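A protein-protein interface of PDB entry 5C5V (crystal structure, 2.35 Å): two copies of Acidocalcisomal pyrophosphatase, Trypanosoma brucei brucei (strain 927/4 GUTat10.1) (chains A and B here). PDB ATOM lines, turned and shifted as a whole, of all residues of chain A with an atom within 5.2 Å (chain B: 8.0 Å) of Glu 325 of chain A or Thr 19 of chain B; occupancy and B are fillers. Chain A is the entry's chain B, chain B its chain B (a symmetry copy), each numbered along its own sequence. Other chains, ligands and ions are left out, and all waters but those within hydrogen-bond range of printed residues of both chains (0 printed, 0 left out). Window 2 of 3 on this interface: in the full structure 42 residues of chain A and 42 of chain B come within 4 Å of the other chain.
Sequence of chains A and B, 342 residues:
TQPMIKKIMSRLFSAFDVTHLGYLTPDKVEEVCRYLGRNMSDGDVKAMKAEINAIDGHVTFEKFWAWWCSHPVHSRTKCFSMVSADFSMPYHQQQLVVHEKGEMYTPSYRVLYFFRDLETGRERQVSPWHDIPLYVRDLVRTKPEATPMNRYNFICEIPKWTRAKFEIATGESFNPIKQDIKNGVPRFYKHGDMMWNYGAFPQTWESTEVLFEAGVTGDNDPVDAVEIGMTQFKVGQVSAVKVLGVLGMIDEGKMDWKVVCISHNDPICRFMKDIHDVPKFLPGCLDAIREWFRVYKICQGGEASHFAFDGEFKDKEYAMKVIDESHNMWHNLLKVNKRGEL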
ATOM      1  N   VAL A 210     -21.672  13.717  12.773  1.00  0.00           N
ATOM      2  CA  VAL A 210     -20.298  14.144  13.007  1.00  0.00           C
ATOM      3  C   VAL A 210     -20.039  14.470  14.461  1.00  0.00           C
ATOM      4  O   VAL A 210     -20.796  15.203  15.092  1.00  0.00           O
ATOM      5  CB  VAL A 210     -19.929  15.390  12.174  1.00  0.00           C
ATOM      6  CG1 VAL A 210     -18.664  16.066  12.741  1.00  0.00           C
ATOM      7  CG2 VAL A 210     -19.780  15.030  10.691  1.00  0.00           C
ATOM      8  N   MET A 320     -13.727  29.943   7.666  1.00  0.00           N
ATOM      9  CA  MET A 320     -13.922  29.434   6.316  1.00  0.00           C
ATOM     10  C   MET A 320     -13.696  27.934   6.265  1.00  0.00           C
ATOM     11  O   MET A 320     -14.317  27.248   5.462  1.00  0.00           O
ATOM     12  CB  MET A 320     -13.020  30.177   5.325  1.00  0.00           C
ATOM     13  CG  MET A 320     -13.481  31.631   5.151  1.00  0.00           C
ATOM     14  SD  MET A 320     -12.640  32.616   3.889  1.00  0.00           S
ATOM     15  CE  MET A 320     -11.156  33.096   4.768  1.00  0.00           C
ATOM     16  N   LYS A 321     -12.834  27.414   7.134  1.00  0.00           N
ATOM     17  CA  LYS A 321     -12.646  25.963   7.224  1.00  0.00           C
ATOM     18  C   LYS A 321     -13.915  25.291   7.744  1.00  0.00           C
ATOM     19  O   LYS A 321     -14.327  24.247   7.239  1.00  0.00           O
ATOM     20  CB  LYS A 321     -11.463  25.616   8.124  1.00  0.00           C
ATOM     21  CG  LYS A 321     -10.105  25.790   7.464  1.00  0.00           C
ATOM     22  CD  LYS A 321      -8.989  25.441   8.444  1.00  0.00           C
ATOM     23  CE  LYS A 321      -7.602  25.409   7.760  1.00  0.00           C
ATOM     24  NZ  LYS A 321      -7.089  26.804   7.407  1.00  0.00           N
ATOM     25  N   VAL A 322     -14.504  25.876   8.783  1.00  0.00           N
ATOM     26  CA  VAL A 322     -15.739  25.355   9.346  1.00  0.00           C
ATOM     27  C   VAL A 322     -16.823  25.325   8.277  1.00  0.00           C
ATOM     28  O   VAL A 322     -17.550  24.347   8.144  1.00  0.00           O
ATOM     29  CB  VAL A 322     -16.216  26.191  10.552  1.00  0.00           C
ATOM     30  CG1 VAL A 322     -17.667  25.893  10.880  1.00  0.00           C
ATOM     31  CG2 VAL A 322     -15.317  25.930  11.767  1.00  0.00           C
ATOM     32  N   ILE A 323     -16.912  26.400   7.505  1.00  0.00           N
ATOM     33  CA  ILE A 323     -17.905  26.486   6.450  1.00  0.00           C
ATOM     34  C   ILE A 323     -17.632  25.457   5.337  1.00  0.00           C
ATOM     35  O   ILE A 323     -18.561  24.792   4.852  1.00  0.00           O
ATOM     36  CB  ILE A 323     -17.954  27.899   5.856  1.00  0.00           C
ATOM     37  CG1 ILE A 323     -18.535  28.881   6.878  1.00  0.00           C
ATOM     38  CG2 ILE A 323     -18.760  27.910   4.549  1.00  0.00           C
ATOM     39  CD1 ILE A 323     -18.386  30.336   6.489  1.00  0.00           C
ATOM     40  N   ASP A 324     -16.365  25.330   4.940  1.00  0.00           N
ATOM     41  CA  ASP A 324     -15.991  24.373   3.907  1.00  0.00           C
ATOM     42  C   ASP A 324     -16.386  22.971   4.348  1.00  0.00           C
ATOM     43  O   ASP A 324     -17.003  22.221   3.594  1.00  0.00           O
ATOM     44  CB  ASP A 324     -14.490  24.434   3.603  1.00  0.00           C
ATOM     45  CG  ASP A 324     -14.056  23.372   2.584  1.00  0.00           C
ATOM     46  OD1 ASP A 324     -14.612  23.336   1.462  1.00  0.00           O
ATOM     47  OD2 ASP A 324     -13.172  22.552   2.902  1.00  0.00           O
ATOM     48  N   GLU A 325     -16.052  22.635   5.587  1.00  0.00           N
ATOM     49  CA  GLU A 325     -16.362  21.324   6.128  1.00  0.00           C
ATOM     50  C   GLU A 325     -17.872  21.076   6.258  1.00  0.00           C
ATOM     51  O   GLU A 325     -18.327  19.950   6.038  1.00  0.00           O
ATOM     52  CB  GLU A 325     -15.675  21.136   7.478  1.00  0.00           C
ATOM     53  CG  GLU A 325     -14.152  21.075   7.361  1.00  0.00           C
ATOM     54  CD  GLU A 325     -13.445  20.942   8.703  1.00  0.00           C
ATOM     55  OE1 GLU A 325     -14.124  20.893   9.761  1.00  0.00           O
ATOM     56  OE2 GLU A 325     -12.191  20.877   8.706  1.00  0.00           O
ATOM     57  N   SER A 326     -18.653  22.102   6.600  1.00  0.00           N
ATOM     58  CA  SER A 326     -20.103  21.915   6.659  1.00  0.00           C
ATOM     59  C   SER A 326     -20.714  21.835   5.247  1.00  0.00           C
ATOM     60  O   SER A 326     -21.810  21.316   5.065  1.00  0.00           O
ATOM     61  CB  SER A 326     -20.774  23.028   7.444  1.00  0.00           C
ATOM     62  OG  SER A 326     -20.777  24.206   6.670  1.00  0.00           O
ATOM     63  N   HIS A 327     -19.992  22.365   4.266  1.00  0.00           N
ATOM     64  CA  HIS A 327     -20.360  22.248   2.865  1.00  0.00           C
ATOM     65  C   HIS A 327     -20.155  20.794   2.412  1.00  0.00           C
ATOM     66  O   HIS A 327     -20.980  20.242   1.689  1.00  0.00           O
ATOM     67  CB  HIS A 327     -19.525  23.210   2.018  1.00  0.00           C
ATOM     68  CG  HIS A 327     -20.033  23.407   0.620  1.00  0.00           C
ATOM     69  ND1 HIS A 327     -21.353  23.679   0.334  1.00  0.00           N
ATOM     70  CD2 HIS A 327     -19.386  23.384  -0.572  1.00  0.00           C
ATOM     71  CE1 HIS A 327     -21.497  23.820  -0.973  1.00  0.00           C
ATOM     72  NE2 HIS A 327     -20.320  23.642  -1.544  1.00  0.00           N
ATOM     73  N   ASN A 328     -19.054  20.186   2.847  1.00  0.00           N
ATOM     74  CA  ASN A 328     -18.799  18.766   2.579  1.00  0.00           C
ATOM     75  C   ASN A 328     -19.901  17.887   3.163  1.00  0.00           C
ATOM     76  O   ASN A 328     -20.381  16.971   2.505  1.00  0.00           O
ATOM     77  CB  ASN A 328     -17.438  18.331   3.142  1.00  0.00           C
ATOM     78  CG  ASN A 328     -16.265  18.962   2.407  1.00  0.00           C
ATOM     79  OD1 ASN A 328     -16.366  19.316   1.243  1.00  0.00           O
ATOM     80  ND2 ASN A 328     -15.146  19.105   3.094  1.00  0.00           N
ATOM     81  N   MET A 329     -20.294  18.183   4.399  1.00  0.00           N
ATOM     82  CA  MET A 329     -21.363  17.459   5.081  1.00  0.00           C
ATOM     83  C   MET A 329     -22.666  17.591   4.325  1.00  0.00           C
ATOM     84  O   MET A 329     -23.430  16.636   4.218  1.00  0.00           O
ATOM     85  CB  MET A 329     -21.568  17.975   6.516  1.00  0.00           C
ATOM     86  CG  MET A 329     -20.378  17.800   7.438  1.00  0.00           C
ATOM     87  SD  MET A 329     -20.485  18.824   8.940  1.00  0.00           S
ATOM     88  CE  MET A 329     -18.840  18.538   9.584  1.00  0.00           C
ATOM     89  N   PHE B  13     -14.526  12.945  -2.928  1.00  0.00           N
ATOM     90  CA  PHE B  13     -13.741  12.409  -1.826  1.00  0.00           C
ATOM     91  C   PHE B  13     -14.015  13.200  -0.534  1.00  0.00           C
ATOM     92  O   PHE B  13     -14.209  12.622   0.536  1.00  0.00           O
ATOM     93  CB  PHE B  13     -12.256  12.457  -2.201  1.00  0.00           C
ATOM     94  CG  PHE B  13     -11.336  11.842  -1.185  1.00  0.00           C
ATOM     95  CD1 PHE B  13     -10.900  12.577  -0.093  1.00  0.00           C
ATOM     96  CD2 PHE B  13     -10.860  10.547  -1.349  1.00  0.00           C
ATOM     97  CE1 PHE B  13     -10.036  12.024   0.838  1.00  0.00           C
ATOM     98  CE2 PHE B  13      -9.987   9.995  -0.430  1.00  0.00           C
ATOM     99  CZ  PHE B  13      -9.580  10.725   0.671  1.00  0.00           C
ATOM    100  N   SER B  14     -14.061  14.521  -0.648  1.00  0.00           N
ATOM    101  CA  SER B  14     -14.299  15.344   0.526  1.00  0.00           C
ATOM    102  C   SER B  14     -15.666  15.095   1.141  1.00  0.00           C
ATOM    103  O   SER B  14     -15.847  15.282   2.346  1.00  0.00           O
ATOM    104  CB  SER B  14     -14.152  16.825   0.188  1.00  0.00           C
ATOM    105  OG  SER B  14     -12.808  17.128  -0.117  1.00  0.00           O
ATOM    106  N   ALA B  15     -16.617  14.641   0.333  1.00  0.00           N
ATOM    107  CA  ALA B  15     -17.955  14.387   0.844  1.00  0.00           C
ATOM    108  C   ALA B  15     -17.988  13.140   1.717  1.00  0.00           C
ATOM    109  O   ALA B  15     -19.005  12.850   2.338  1.00  0.00           O
ATOM    110  CB  ALA B  15     -18.944  14.266  -0.294  1.00  0.00           C
ATOM    111  N   PHE B  16     -16.881  12.401   1.757  1.00  0.00           N
ATOM    112  CA  PHE B  16     -16.771  11.227   2.621  1.00  0.00           C
ATOM    113  C   PHE B  16     -15.657  11.373   3.655  1.00  0.00           C
ATOM    114  O   PHE B  16     -15.469  10.512   4.502  1.00  0.00           O
ATOM    115  CB  PHE B  16     -16.536   9.972   1.781  1.00  0.00           C
ATOM    116  CG  PHE B  16     -17.690   9.617   0.898  1.00  0.00           C
ATOM    117  CD1 PHE B  16     -18.726   8.833   1.372  1.00  0.00           C
ATOM    118  CD2 PHE B  16     -17.754  10.089  -0.403  1.00  0.00           C
ATOM    119  CE1 PHE B  16     -19.796   8.515   0.568  1.00  0.00           C
ATOM    120  CE2 PHE B  16     -18.824   9.762  -1.215  1.00  0.00           C
ATOM    121  CZ  PHE B  16     -19.844   8.976  -0.725  1.00  0.00           C
ATOM    122  N   ASP B  17     -14.918  12.463   3.567  1.00  0.00           N
ATOM    123  CA  ASP B  17     -13.896  12.825   4.538  1.00  0.00           C
ATOM    124  C   ASP B  17     -14.167  14.281   4.875  1.00  0.00           C
ATOM    125  O   ASP B  17     -13.371  15.159   4.568  1.00  0.00           O
ATOM    126  CB  ASP B  17     -12.491  12.630   3.956  1.00  0.00           C
ATOM    127  CG  ASP B  17     -11.384  13.125   4.883  1.00  0.00           C
ATOM    128  OD1 ASP B  17     -11.532  12.985   6.111  1.00  0.00           O
ATOM    129  OD2 ASP B  17     -10.373  13.671   4.383  1.00  0.00           O
ATOM    130  N   VAL B  18     -15.321  14.529   5.484  1.00  0.00           N
ATOM    131  CA  VAL B  18     -15.859  15.891   5.591  1.00  0.00           C
ATOM    132  C   VAL B  18     -15.006  16.810   6.465  1.00  0.00           C
ATOM    133  O   VAL B  18     -14.933  18.007   6.210  1.00  0.00           O
ATOM    134  CB  VAL B  18     -17.308  15.863   6.126  1.00  0.00           C
ATOM    135  CG1 VAL B  18     -18.225  15.142   5.132  1.00  0.00           C
ATOM    136  CG2 VAL B  18     -17.364  15.186   7.478  1.00  0.00           C
ATOM    137  N   THR B  19     -14.328  16.242   7.459  1.00  0.00           N
ATOM    138  CA  THR B  19     -13.495  17.029   8.361  1.00  0.00           C
ATOM    139  C   THR B  19     -12.035  17.035   7.911  1.00  0.00           C
ATOM    140  O   THR B  19     -11.163  17.509   8.632  1.00  0.00           O
ATOM    141  CB  THR B  19     -13.567  16.534   9.813  1.00  0.00           C
ATOM    142  OG1 THR B  19     -13.041  15.210   9.893  1.00  0.00           O
ATOM    143  CG2 THR B  19     -14.997  16.529  10.303  1.00  0.00           C
ATOM    144  N   HIS B  20     -11.767  16.498   6.723  1.00  0.00           N
ATOM    145  CA  HIS B  20     -10.407  16.486   6.175  1.00  0.00           C
ATOM    146  C   HIS B  20      -9.375  15.763   7.056  1.00  0.00           C
ATOM    147  O   HIS B  20      -8.305  16.305   7.316  1.00  0.00           O
ATOM    148  CB  HIS B  20      -9.925  17.925   5.919  1.00  0.00           C
ATOM    149  CG  HIS B  20     -10.684  18.648   4.846  1.00  0.00           C
ATOM    150  ND1 HIS B  20     -11.126  18.032   3.690  1.00  0.00           N
ATOM    151  CD2 HIS B  20     -11.091  19.941   4.758  1.00  0.00           C
ATOM    152  CE1 HIS B  20     -11.763  18.914   2.938  1.00  0.00           C
ATOM    153  NE2 HIS B  20     -11.758  20.080   3.566  1.00  0.00           N
ATOM    154  N   LEU B  21      -9.699  14.555   7.510  1.00  0.00           N
ATOM    155  CA  LEU B  21      -8.703  13.677   8.111  1.00  0.00           C
ATOM    156  C   LEU B  21      -7.568  13.421   7.142  1.00  0.00           C
ATOM    157  O   LEU B  21      -6.455  13.103   7.562  1.00  0.00           O
ATOM    158  CB  LEU B  21      -9.306  12.328   8.529  1.00  0.00           C
ATOM    159  CG  LEU B  21     -10.319  12.213   9.656  1.00  0.00           C
ATOM    160  CD1 LEU B  21     -10.807  10.784   9.745  1.00  0.00           C
ATOM    161  CD2 LEU B  21      -9.628  12.595  10.970  1.00  0.00           C
ATOM    162  N   GLY B  22      -7.871  13.522   5.851  1.00  0.00           N
ATOM    163  CA  GLY B  22      -6.911  13.272   4.793  1.00  0.00           C
ATOM    164  C   GLY B  22      -7.008  11.886   4.205  1.00  0.00           C
ATOM    165  O   GLY B  22      -6.295  11.567   3.253  1.00  0.00           O
ATOM    166  N   TYR B  23      -7.873  11.046   4.771  1.00  0.00           N
ATOM    167  CA  TYR B  23      -8.050   9.685   4.279  1.00  0.00           C
ATOM    168  C   TYR B  23      -9.447   9.174   4.614  1.00  0.00           C
ATOM    169  O   TYR B  23     -10.176   9.801   5.390  1.00  0.00           O
ATOM    170  CB  TYR B  23      -7.025   8.742   4.892  1.00  0.00           C
ATOM    171  CG  TYR B  23      -7.128   8.644   6.401  1.00  0.00           C
ATOM    172  CD1 TYR B  23      -7.915   7.671   6.992  1.00  0.00           C
ATOM    173  CD2 TYR B  23      -6.480   9.557   7.228  1.00  0.00           C
ATOM    174  CE1 TYR B  23      -8.027   7.576   8.350  1.00  0.00           C
ATOM    175  CE2 TYR B  23      -6.583   9.475   8.595  1.00  0.00           C
ATOM    176  CZ  TYR B  23      -7.364   8.489   9.152  1.00  0.00           C
ATOM    177  OH  TYR B  23      -7.483   8.392  10.519  1.00  0.00           O
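The side-chain carboxylate (OD2) of Asp 324 of chain A sits at hydrogen-bond distance from a ring nitrogen (NE2) of His 20 of chain B (2.9 Å).
The backbone carbonyl oxygen of Val 18 of chain B sits at hydrogen-bond distance from the side-chain amide nitrogen of Asn 328 of chain A, 3.3 Å away.
Among the printed residues, merely in contact across the chains: Glu 325 of chain A with Val 18 of chain B, Glu 325 of chain A with Thr 19 of chain B, Asn 328 of chain A with Ser 14 of chain B, Asn 328 of chain A with Ala 15 of chain B, Asn 328 of chain A with His 20 of chain B and Met 329 of chain A with Val 18 of chain B.
Of chain B, only Val 18 (3.4 Å) and Thr 19 (3.5 Å) come within 4 Å of Glu 325 of chain A.
Printed residues of chain B within 4 Å of Met 329 of chain A: Val 18.
Of the printed residues of chain A, Ser 14 of chain B touches Asn 328.
Of the printed residues of chain A, Thr 19 of chain B touches Glu 325 (3.5 Å).
Of the printed residues of chain A, His 20 of chain B touches Asp 324 and Asn 328.
The nearest residue of chain B that does not touch Glu 325 of chain A is His 20 of chain B (4.2 Å).
The nearest printed residue of chain B that does not touch Met 329 of chain A is Thr 19 of chain B (4.4 Å).
Hydrophobic or aromatic side chains of chain B within 4 Å of the printed part of chain A: Val 18 and His 20.
Of the 11 printed residues of chain A, 4 touch a printed residue of chain B.
Hydrophobic or aromatic side chains of chain A that line the printed part of chain B: Met 329.
Among the printed residues, no Asp or Glu carboxylate lies within 4 Å of a Lys or Arg side-chain nitrogen of the other chain.
No position is printed for both chains.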
